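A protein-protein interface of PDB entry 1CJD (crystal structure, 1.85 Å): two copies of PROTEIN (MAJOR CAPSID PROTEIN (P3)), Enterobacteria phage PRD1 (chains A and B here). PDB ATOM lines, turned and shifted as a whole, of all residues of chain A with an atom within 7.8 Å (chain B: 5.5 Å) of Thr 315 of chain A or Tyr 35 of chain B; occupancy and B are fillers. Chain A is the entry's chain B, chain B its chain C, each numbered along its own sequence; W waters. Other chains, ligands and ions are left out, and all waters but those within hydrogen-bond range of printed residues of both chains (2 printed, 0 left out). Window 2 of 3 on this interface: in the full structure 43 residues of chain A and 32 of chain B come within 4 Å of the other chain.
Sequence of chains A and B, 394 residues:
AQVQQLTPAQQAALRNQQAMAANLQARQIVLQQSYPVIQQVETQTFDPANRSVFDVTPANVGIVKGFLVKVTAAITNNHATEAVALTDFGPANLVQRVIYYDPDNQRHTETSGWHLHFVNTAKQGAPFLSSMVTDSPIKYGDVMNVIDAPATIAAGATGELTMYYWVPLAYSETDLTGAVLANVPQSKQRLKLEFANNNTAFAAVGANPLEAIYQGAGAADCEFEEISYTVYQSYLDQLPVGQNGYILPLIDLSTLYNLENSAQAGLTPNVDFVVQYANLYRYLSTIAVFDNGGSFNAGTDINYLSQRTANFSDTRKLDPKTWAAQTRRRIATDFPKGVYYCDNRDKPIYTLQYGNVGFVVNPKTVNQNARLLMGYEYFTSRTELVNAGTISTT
O of Thr 315 of chain A sits at hydrogen-bond distance from N of Ile 38 of chain B, at 3.2 Å. NZ of Lys 347 of chain A is in hydrogen-bond range of O of Ser 34 of chain B (3.4 Å).
N of Thr 315 of chain A is in hydrogen-bond range of O of Gln 307 of chain A, 3.0 Å away. The side-chain amide oxygen of Gln 307 of chain A is in hydrogen-bond range of the side-chain amide nitrogen of Asn 344 of chain A, 2.9 Å away. The side-chain amide nitrogen of Asn 344 of chain A sits at hydrogen-bond distance from the side-chain sulfur of Cys 342 of chain A, 3.6 Å away. N of Tyr 35 of chain B is in hydrogen-bond range of O of Asp 237 of chain B (2.7 Å). O of Tyr 235 of chain B is in hydrogen-bond range of N of Val 37 of chain B (2.8 Å).
Among the printed residues, merely in contact across the chains: Thr 315 of chain A with Tyr 35 of chain B, Arg 316 of chain A with Ile 38 of chain B, Thr 315 of chain A with Val 37 of chain B, Lys 347 of chain A with Pro 36 of chain B, Asn 344 of chain A with Tyr 35 of chain B, Leu 318 of chain A with Ile 38 of chain B and Thr 315 of chain A with Pro 36 of chain B.
Of the printed residues of chain B, Thr 315 of chain A touches Tyr 35, Pro 36, Val 37 and Ile 38. Ser 34 of chain B touches just one residue of chain A: Lys 347 (3.4 Å). Printed residues of chain A within 4 Å of Val 37 of chain B: Thr 315. Of the printed residues of chain A, Ile 38 of chain B touches Thr 315 (3.2 Å), Arg 316 (3.5 Å) and Leu 318 (3.99 Å). Asp 237 of chain B touches none of the printed residues of chain A. The nearest printed residue of chain A that does not touch Tyr 35 of chain B is Lys 347 of chain A (4.04 Å).
Hydrophobic or aromatic side chains of chain B that line the printed part of chain A: Tyr 35, Pro 36, Val 37 and Ile 38. Of the 22 printed residues of chain A, 5 touch a printed residue of chain B. Printed residues of chain A that touch a printed residue of chain B: Thr 315, Arg 316, Leu 318, Asn 344 and Lys 347. Among the printed residues, 9 pairs touch across the chains.
No position is printed for both chains.
Water W1 bridges O of Thr 315 of chain A (2.7 Å) and O of Pro 36 of chain B (3.1 Å). Water W2 lies within hydrogen-bond range of the backbone carbonyl oxygen of Asp 314 of chain A (2.8 Å), the backbone NH of Lys 317 of chain A (2.9 Å), the backbone carbonyl oxygen of Ile 38 of chain B (3.1 Å) and the backbone NH of Arg 316 of chain A (3.1 Å).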
ATOM      1  N   SER A 306      34.986  32.517  10.797  1.00  0.00           N
ATOM      2  CA  SER A 306      33.587  32.214  10.918  1.00  0.00           C
ATOM      3  C   SER A 306      33.348  30.736  11.086  1.00  0.00           C
ATOM      4  O   SER A 306      34.268  29.919  10.995  1.00  0.00           O
ATOM      5  CB  SER A 306      32.857  32.703   9.670  1.00  0.00           C
ATOM      6  OG  SER A 306      31.459  32.680   9.882  1.00  0.00           O
ATOM      7  N   GLN A 307      32.086  30.420  11.360  1.00  0.00           N
ATOM      8  CA  GLN A 307      31.599  29.051  11.467  1.00  0.00           C
ATOM      9  C   GLN A 307      30.350  29.158  10.603  1.00  0.00           C
ATOM     10  O   GLN A 307      29.552  30.071  10.770  1.00  0.00           O
ATOM     11  CB  GLN A 307      31.251  28.681  12.912  1.00  0.00           C
ATOM     12  CG  GLN A 307      32.413  28.066  13.672  1.00  0.00           C
ATOM     13  CD  GLN A 307      31.991  27.403  14.984  1.00  0.00           C
ATOM     14  OE1 GLN A 307      32.655  26.307  15.338  1.00  0.00           O
ATOM     15  NE2 GLN A 307      31.080  27.877  15.671  1.00  0.00           N
ATOM     16  N   ARG A 308      30.199  28.273   9.638  1.00  0.00           N
ATOM     17  CA  ARG A 308      29.038  28.377   8.790  1.00  0.00           C
ATOM     18  C   ARG A 308      28.516  27.048   8.297  1.00  0.00           C
ATOM     19  O   ARG A 308      29.190  26.017   8.399  1.00  0.00           O
ATOM     20  CB  ARG A 308      29.357  29.273   7.594  1.00  0.00           C
ATOM     21  CG  ARG A 308      30.007  28.566   6.416  1.00  0.00           C
ATOM     22  CD  ARG A 308      29.855  29.392   5.136  1.00  0.00           C
ATOM     23  NE  ARG A 308      30.314  30.770   5.337  1.00  0.00           N
ATOM     24  CZ  ARG A 308      31.358  31.326   4.714  1.00  0.00           C
ATOM     25  NH1 ARG A 308      32.066  30.612   3.829  1.00  0.00           N
ATOM     26  NH2 ARG A 308      31.704  32.591   4.985  1.00  0.00           N
ATOM     27  N   THR A 309      27.292  27.092   7.784  1.00  0.00           N
ATOM     28  CA  THR A 309      26.640  25.930   7.198  1.00  0.00           C
ATOM     29  C   THR A 309      26.688  26.123   5.684  1.00  0.00           C
ATOM     30  O   THR A 309      26.448  27.241   5.212  1.00  0.00           O
ATOM     31  CB  THR A 309      25.194  25.864   7.584  1.00  0.00           C
ATOM     32  OG1 THR A 309      25.109  25.646   8.994  1.00  0.00           O
ATOM     33  CG2 THR A 309      24.495  24.725   6.812  1.00  0.00           C
ATOM     34  N   PHE A 312      25.202  28.639   3.297  1.00  0.00           N
ATOM     35  CA  PHE A 312      25.717  30.050   3.341  1.00  0.00           C
ATOM     36  C   PHE A 312      25.481  30.837   4.650  1.00  0.00           C
ATOM     37  O   PHE A 312      25.843  32.062   4.770  1.00  0.00           O
ATOM     38  CB  PHE A 312      25.128  30.864   2.151  1.00  0.00           C
ATOM     39  N   SER A 313      24.887  30.166   5.630  1.00  0.00           N
ATOM     40  CA  SER A 313      24.586  30.794   6.899  1.00  0.00           C
ATOM     41  C   SER A 313      25.777  30.758   7.880  1.00  0.00           C
ATOM     42  O   SER A 313      26.133  29.688   8.404  1.00  0.00           O
ATOM     43  CB  SER A 313      23.348  30.108   7.507  1.00  0.00           C
ATOM     44  OG  SER A 313      23.075  28.859   6.858  1.00  0.00           O
ATOM     45  N   ASP A 314      26.407  31.921   8.086  1.00  0.00           N
ATOM     46  CA  ASP A 314      27.509  32.060   9.051  1.00  0.00           C
ATOM     47  C   ASP A 314      26.806  32.392  10.376  1.00  0.00           C
ATOM     48  O   ASP A 314      25.981  33.311  10.432  1.00  0.00           O
ATOM     49  CB  ASP A 314      28.440  33.229   8.697  1.00  0.00           C
ATOM     50  CG  ASP A 314      29.229  32.991   7.433  1.00  0.00           C
ATOM     51  OD1 ASP A 314      28.704  33.322   6.349  1.00  0.00           O
ATOM     52  OD2 ASP A 314      30.366  32.485   7.508  1.00  0.00           O
ATOM     53  N   THR A 315      27.104  31.650  11.437  1.00  0.00           N
ATOM     54  CA  THR A 315      26.464  31.934  12.711  1.00  0.00           C
ATOM     55  C   THR A 315      27.323  32.872  13.558  1.00  0.00           C
ATOM     56  O   THR A 315      26.933  33.238  14.684  1.00  0.00           O
ATOM     57  CB  THR A 315      26.219  30.663  13.525  1.00  0.00           C
ATOM     58  OG1 THR A 315      27.455  29.940  13.626  1.00  0.00           O
ATOM     59  CG2 THR A 315      25.110  29.806  12.887  1.00  0.00           C
ATOM     60  N   ARG A 316      28.497  33.246  13.044  1.00  0.00           N
ATOM     61  CA  ARG A 316      29.363  34.157  13.786  1.00  0.00           C
ATOM     62  C   ARG A 316      30.542  34.624  12.949  1.00  0.00           C
ATOM     63  O   ARG A 316      31.699  34.402  13.299  1.00  0.00           O
ATOM     64  CB  ARG A 316      29.851  33.516  15.111  1.00  0.00           C
ATOM     65  CG  ARG A 316      30.600  32.152  15.006  1.00  0.00           C
ATOM     66  CD  ARG A 316      31.097  31.688  16.396  1.00  0.00           C
ATOM     67  NE  ARG A 316      32.255  32.476  16.834  1.00  0.00           N
ATOM     68  CZ  ARG A 316      32.752  32.527  18.073  1.00  0.00           C
ATOM     69  NH1 ARG A 316      32.195  31.828  19.047  1.00  0.00           N
ATOM     70  NH2 ARG A 316      33.833  33.264  18.331  1.00  0.00           N
ATOM     71  N   LYS A 317      30.246  35.253  11.822  1.00  0.00           N
ATOM     72  CA  LYS A 317      31.311  35.781  10.972  1.00  0.00           C
ATOM     73  C   LYS A 317      31.855  37.049  11.669  1.00  0.00           C
ATOM     74  O   LYS A 317      31.140  38.046  11.770  1.00  0.00           O
ATOM     75  CB  LYS A 317      30.737  36.127   9.614  1.00  0.00           C
ATOM     76  CG  LYS A 317      31.761  36.636   8.650  1.00  0.00           C
ATOM     77  CD  LYS A 317      31.213  36.560   7.252  1.00  0.00           C
ATOM     78  CE  LYS A 317      31.843  37.600   6.375  1.00  0.00           C
ATOM     79  NZ  LYS A 317      30.782  38.344   5.649  1.00  0.00           N
ATOM     80  N   LEU A 318      33.098  37.016  12.147  1.00  0.00           N
ATOM     81  CA  LEU A 318      33.662  38.154  12.874  1.00  0.00           C
ATOM     82  C   LEU A 318      35.086  38.579  12.476  1.00  0.00           C
ATOM     83  O   LEU A 318      35.901  37.747  12.051  1.00  0.00           O
ATOM     84  CB  LEU A 318      33.662  37.860  14.377  1.00  0.00           C
ATOM     85  CG  LEU A 318      32.418  37.241  14.998  1.00  0.00           C
ATOM     86  CD1 LEU A 318      32.718  36.735  16.412  1.00  0.00           C
ATOM     87  CD2 LEU A 318      31.348  38.293  15.068  1.00  0.00           C
ATOM     88  N   TRP A 323      36.377  38.543  17.322  1.00  0.00           N
ATOM     89  CA  TRP A 323      36.496  37.116  17.584  1.00  0.00           C
ATOM     90  C   TRP A 323      37.314  36.970  18.900  1.00  0.00           C
ATOM     91  O   TRP A 323      36.965  36.202  19.813  1.00  0.00           O
ATOM     92  CB  TRP A 323      37.224  36.452  16.416  1.00  0.00           C
ATOM     93  CG  TRP A 323      37.329  34.956  16.555  1.00  0.00           C
ATOM     94  CD1 TRP A 323      38.234  34.263  17.312  1.00  0.00           C
ATOM     95  CD2 TRP A 323      36.512  33.981  15.911  1.00  0.00           C
ATOM     96  NE1 TRP A 323      38.027  32.918  17.179  1.00  0.00           N
ATOM     97  CE2 TRP A 323      36.976  32.714  16.322  1.00  0.00           C
ATOM     98  CE3 TRP A 323      35.430  34.052  15.027  1.00  0.00           C
ATOM     99  CZ2 TRP A 323      36.392  31.520  15.873  1.00  0.00           C
ATOM    100  CZ3 TRP A 323      34.847  32.867  14.583  1.00  0.00           C
ATOM    101  CH2 TRP A 323      35.333  31.619  15.008  1.00  0.00           C
ATOM    102  N   CYS A 342      37.352  28.771  19.608  1.00  0.00           N
ATOM    103  CA  CYS A 342      35.926  28.807  19.370  1.00  0.00           C
ATOM    104  C   CYS A 342      35.263  27.838  20.331  1.00  0.00           C
ATOM    105  O   CYS A 342      35.553  26.648  20.298  1.00  0.00           O
ATOM    106  CB  CYS A 342      35.640  28.380  17.926  1.00  0.00           C
ATOM    107  SG  CYS A 342      33.985  28.664  17.475  1.00  0.00           S
ATOM    108  N   ASP A 343      34.372  28.343  21.181  1.00  0.00           N
ATOM    109  CA  ASP A 343      33.663  27.514  22.158  1.00  0.00           C
ATOM    110  C   ASP A 343      32.276  27.104  21.607  1.00  0.00           C
ATOM    111  O   ASP A 343      31.489  27.968  21.247  1.00  0.00           O
ATOM    112  CB  ASP A 343      33.524  28.333  23.464  1.00  0.00           C
ATOM    113  CG  ASP A 343      32.673  27.640  24.544  1.00  0.00           C
ATOM    114  OD1 ASP A 343      31.699  26.926  24.233  1.00  0.00           O
ATOM    115  OD2 ASP A 343      32.977  27.829  25.739  1.00  0.00           O
ATOM    116  N   ASN A 344      31.995  25.800  21.519  1.00  0.00           N
ATOM    117  CA  ASN A 344      30.682  25.290  21.067  1.00  0.00           C
ATOM    118  C   ASN A 344      30.232  24.248  22.082  1.00  0.00           C
ATOM    119  O   ASN A 344      29.544  23.286  21.741  1.00  0.00           O
ATOM    120  CB  ASN A 344      30.775  24.611  19.701  1.00  0.00           C
ATOM    121  CG  ASN A 344      31.139  25.574  18.590  1.00  0.00           C
ATOM    122  OD1 ASN A 344      30.307  26.371  18.127  1.00  0.00           O
ATOM    123  ND2 ASN A 344      32.383  25.508  18.150  1.00  0.00           N
ATOM    124  N   ASP A 346      28.069  24.330  24.679  1.00  0.00           N
ATOM    125  CA  ASP A 346      26.656  24.169  24.967  1.00  0.00           C
ATOM    126  C   ASP A 346      25.896  23.529  23.803  1.00  0.00           C
ATOM    127  O   ASP A 346      24.945  22.775  24.007  1.00  0.00           O
ATOM    128  CB  ASP A 346      26.062  25.529  25.347  1.00  0.00           C
ATOM    129  CG  ASP A 346      26.669  26.086  26.642  1.00  0.00           C
ATOM    130  OD1 ASP A 346      27.011  25.287  27.548  1.00  0.00           O
ATOM    131  OD2 ASP A 346      26.819  27.324  26.757  1.00  0.00           O
ATOM    132  N   LYS A 347      26.324  23.820  22.579  1.00  0.00           N
ATOM    133  CA  LYS A 347      25.691  23.254  21.390  1.00  0.00           C
ATOM    134  C   LYS A 347      26.806  22.793  20.461  1.00  0.00           C
ATOM    135  O   LYS A 347      27.168  23.498  19.521  1.00  0.00           O
ATOM    136  CB  LYS A 347      24.824  24.320  20.711  1.00  0.00           C
ATOM    137  CG  LYS A 347      23.605  24.732  21.556  1.00  0.00           C
ATOM    138  CD  LYS A 347      22.824  25.878  20.929  1.00  0.00           C
ATOM    139  CE  LYS A 347      21.748  26.396  21.887  1.00  0.00           C
ATOM    140  NZ  LYS A 347      20.456  25.679  21.682  1.00  0.00           N
ATOM    141  N   PRO A 348      27.379  21.609  20.729  1.00  0.00           N
ATOM    142  CA  PRO A 348      28.465  21.039  19.933  1.00  0.00           C
ATOM    143  C   PRO A 348      28.130  21.004  18.461  1.00  0.00           C
ATOM    144  O   PRO A 348      26.963  20.808  18.106  1.00  0.00           O
ATOM    145  CB  PRO A 348      28.619  19.630  20.486  1.00  0.00           C
ATOM    146  CG  PRO A 348      28.090  19.689  21.821  1.00  0.00           C
ATOM    147  CD  PRO A 348      27.008  20.720  21.835  1.00  0.00           C
ATOM    148  N   ILE A 349      29.140  21.211  17.614  1.00  0.00           N
ATOM    149  CA  ILE A 349      28.934  21.137  16.172  1.00  0.00           C
ATOM    150  C   ILE A 349      28.724  19.650  15.917  1.00  0.00           C
ATOM    151  O   ILE A 349      29.533  18.830  16.318  1.00  0.00           O
ATOM    152  CB  ILE A 349      30.161  21.618  15.357  1.00  0.00           C
ATOM    153  CG1 ILE A 349      30.494  23.069  15.705  1.00  0.00           C
ATOM    154  CG2 ILE A 349      29.885  21.450  13.855  1.00  0.00           C
ATOM    155  CD1 ILE A 349      29.347  24.004  15.541  1.00  0.00           C
ATOM    156  N   TYR A 354      22.543  19.433  11.925  1.00  0.00           N
ATOM    157  CA  TYR A 354      22.713  20.764  11.340  1.00  0.00           C
ATOM    158  C   TYR A 354      23.162  20.807   9.874  1.00  0.00           C
ATOM    159  O   TYR A 354      23.123  21.879   9.244  1.00  0.00           O
ATOM    160  CB  TYR A 354      23.701  21.581  12.209  1.00  0.00           C
ATOM    161  N   VAL A 357      29.109  21.552   8.258  1.00  0.00           N
ATOM    162  CA  VAL A 357      29.577  22.786   8.851  1.00  0.00           C
ATOM    163  C   VAL A 357      31.059  22.824   8.592  1.00  0.00           C
ATOM    164  O   VAL A 357      31.713  21.775   8.491  1.00  0.00           O
ATOM    165  CB  VAL A 357      29.364  22.778  10.373  1.00  0.00           C
ATOM    166  CG1 VAL A 357      29.647  24.140  10.956  1.00  0.00           C
ATOM    167  CG2 VAL A 357      27.964  22.345  10.680  1.00  0.00           C
ATOM    168  N   GLY A 358      31.593  24.033   8.477  1.00  0.00           N
ATOM    169  CA  GLY A 358      33.018  24.186   8.253  1.00  0.00           C
ATOM    170  C   GLY A 358      33.518  25.366   9.061  1.00  0.00           C
ATOM    171  O   GLY A 358      32.738  26.252   9.418  1.00  0.00           O
ATOM    172  N   GLN B  33      15.857  25.024  21.363  1.00  0.00           N
ATOM    173  CA  GLN B  33      15.615  24.857  19.915  1.00  0.00           C
ATOM    174  C   GLN B  33      16.186  25.845  18.896  1.00  0.00           C
ATOM    175  O   GLN B  33      16.497  25.458  17.762  1.00  0.00           O
ATOM    176  CB  GLN B  33      14.108  24.766  19.636  1.00  0.00           C
ATOM    177  CG  GLN B  33      13.287  24.107  20.729  1.00  0.00           C
ATOM    178  CD  GLN B  33      13.429  22.603  20.737  1.00  0.00           C
ATOM    179  OE1 GLN B  33      13.787  21.997  19.726  1.00  0.00           O
ATOM    180  NE2 GLN B  33      13.148  21.987  21.884  1.00  0.00           N
ATOM    181  N   SER B  34      16.273  27.119  19.267  1.00  0.00           N
ATOM    182  CA  SER B  34      16.791  28.150  18.356  1.00  0.00           C
ATOM    183  C   SER B  34      18.304  28.129  18.350  1.00  0.00           C
ATOM    184  O   SER B  34      18.931  27.559  19.253  1.00  0.00           O
ATOM    185  CB  SER B  34      16.330  29.532  18.821  1.00  0.00           C
ATOM    186  OG  SER B  34      16.883  29.829  20.093  1.00  0.00           O
ATOM    187  N   TYR B  35      18.908  28.727  17.333  1.00  0.00           N
ATOM    188  CA  TYR B  35      20.368  28.781  17.338  1.00  0.00           C
ATOM    189  C   TYR B  35      20.871  30.207  17.419  1.00  0.00           C
ATOM    190  O   TYR B  35      20.445  31.083  16.653  1.00  0.00           O
ATOM    191  CB  TYR B  35      20.996  28.117  16.110  1.00  0.00           C
ATOM    192  CG  TYR B  35      22.500  27.855  16.304  1.00  0.00           C
ATOM    193  CD1 TYR B  35      22.957  26.692  16.971  1.00  0.00           C
ATOM    194  CD2 TYR B  35      23.470  28.751  15.806  1.00  0.00           C
ATOM    195  CE1 TYR B  35      24.347  26.422  17.131  1.00  0.00           C
ATOM    196  CE2 TYR B  35      24.858  28.490  15.961  1.00  0.00           C
ATOM    197  CZ  TYR B  35      25.286  27.322  16.620  1.00  0.00           C
ATOM    198  OH  TYR B  35      26.638  27.038  16.734  1.00  0.00           O
ATOM    199  N   PRO B  36      21.790  30.457  18.358  1.00  0.00           N
ATOM    200  CA  PRO B  36      22.370  31.786  18.552  1.00  0.00           C
ATOM    201  C   PRO B  36      23.193  32.251  17.339  1.00  0.00           C
ATOM    202  O   PRO B  36      24.001  31.501  16.776  1.00  0.00           O
ATOM    203  CB  PRO B  36      23.232  31.619  19.806  1.00  0.00           C
ATOM    204  CG  PRO B  36      23.569  30.164  19.824  1.00  0.00           C
ATOM    205  CD  PRO B  36      22.340  29.478  19.312  1.00  0.00           C
ATOM    206  N   VAL B  37      22.986  33.498  16.945  1.00  0.00           N
ATOM    207  CA  VAL B  37      23.708  34.069  15.824  1.00  0.00           C
ATOM    208  C   VAL B  37      24.212  35.449  16.215  1.00  0.00           C
ATOM    209  O   VAL B  37      23.572  36.147  16.988  1.00  0.00           O
ATOM    210  CB  VAL B  37      22.779  34.237  14.598  1.00  0.00           C
ATOM    211  CG1 VAL B  37      23.559  34.865  13.431  1.00  0.00           C
ATOM    212  CG2 VAL B  37      22.192  32.898  14.206  1.00  0.00           C
ATOM    213  N   ILE B  38      25.381  35.823  15.724  1.00  0.00           N
ATOM    214  CA  ILE B  38      25.885  37.169  15.951  1.00  0.00           C
ATOM    215  C   ILE B  38      26.404  37.591  14.576  1.00  0.00           C
ATOM    216  O   ILE B  38      27.242  36.907  13.981  1.00  0.00           O
ATOM    217  CB  ILE B  38      27.027  37.265  17.004  1.00  0.00           C
ATOM    218  CG1 ILE B  38      27.482  38.723  17.072  1.00  0.00           C
ATOM    219  CG2 ILE B  38      28.221  36.373  16.632  1.00  0.00           C
ATOM    220  CD1 ILE B  38      28.383  39.031  18.223  1.00  0.00           C
ATOM    221  N   TYR B 235      21.304  37.502  18.152  1.00  0.00           N
ATOM    222  CA  TYR B 235      19.908  37.081  18.227  1.00  0.00           C
ATOM    223  C   TYR B 235      19.726  35.574  18.163  1.00  0.00           C
ATOM    224  O   TYR B 235      20.687  34.824  17.974  1.00  0.00           O
ATOM    225  CB  TYR B 235      19.115  37.717  17.086  1.00  0.00           C
ATOM    226  CG  TYR B 235      19.597  37.319  15.715  1.00  0.00           C
ATOM    227  CD1 TYR B 235      20.635  38.006  15.105  1.00  0.00           C
ATOM    228  CD2 TYR B 235      18.990  36.281  15.008  1.00  0.00           C
ATOM    229  CE1 TYR B 235      21.057  37.680  13.826  1.00  0.00           C
ATOM    230  CE2 TYR B 235      19.393  35.944  13.735  1.00  0.00           C
ATOM    231  CZ  TYR B 235      20.430  36.654  13.144  1.00  0.00           C
ATOM    232  OH  TYR B 235      20.830  36.379  11.853  1.00  0.00           O
ATOM    233  N   LEU B 236      18.478  35.136  18.330  1.00  0.00           N
ATOM    234  CA  LEU B 236      18.160  33.711  18.271  1.00  0.00           C
ATOM    235  C   LEU B 236      17.350  33.444  17.017  1.00  0.00           C
ATOM    236  O   LEU B 236      16.367  34.129  16.715  1.00  0.00           O
ATOM    237  CB  LEU B 236      17.399  33.246  19.528  1.00  0.00           C
ATOM    238  CG  LEU B 236      18.085  33.521  20.875  1.00  0.00           C
ATOM    239  CD1 LEU B 236      17.169  33.109  22.011  1.00  0.00           C
ATOM    240  CD2 LEU B 236      19.414  32.788  20.946  1.00  0.00           C
ATOM    241  N   ASP B 237      17.810  32.446  16.279  1.00  0.00           N
ATOM    242  CA  ASP B 237      17.191  32.036  15.039  1.00  0.00           C
ATOM    243  C   ASP B 237      16.556  30.645  15.165  1.00  0.00           C
ATOM    244  O   ASP B 237      16.821  29.911  16.133  1.00  0.00           O
ATOM    245  CB  ASP B 237      18.257  32.011  13.949  1.00  0.00           C
ATOM    246  CG  ASP B 237      17.783  32.633  12.672  1.00  0.00           C
ATOM    247  OD1 ASP B 237      16.613  33.059  12.615  1.00  0.00           O
ATOM    248  OD2 ASP B 237      18.580  32.696  11.724  1.00  0.00           O
ATOM    249  N   GLN B 238      15.741  30.288  14.167  1.00  0.00           N
ATOM    250  CA  GLN B 238      15.057  28.988  14.130  1.00  0.00           C
ATOM    251  C   GLN B 238      14.216  28.889  15.385  1.00  0.00           C
ATOM    252  O   GLN B 238      14.381  27.946  16.167  1.00  0.00           O
ATOM    253  CB  GLN B 238      16.060  27.845  14.178  1.00  0.00           C
ATOM    254  CG  GLN B 238      16.777  27.507  12.907  1.00  0.00           C
ATOM    255  CD  GLN B 238      17.743  26.335  13.140  1.00  0.00           C
ATOM    256  OE1 GLN B 238      18.141  26.049  14.290  1.00  0.00           O
ATOM    257  NE2 GLN B 238      18.122  25.650  12.058  1.00  0.00           N
HETATM  258  O   HOH W   1      27.011  31.943  17.012  1.00  0.00           O
HETATM  259  O   HOH W   2      27.477  35.574  11.222  1.00  0.00           O
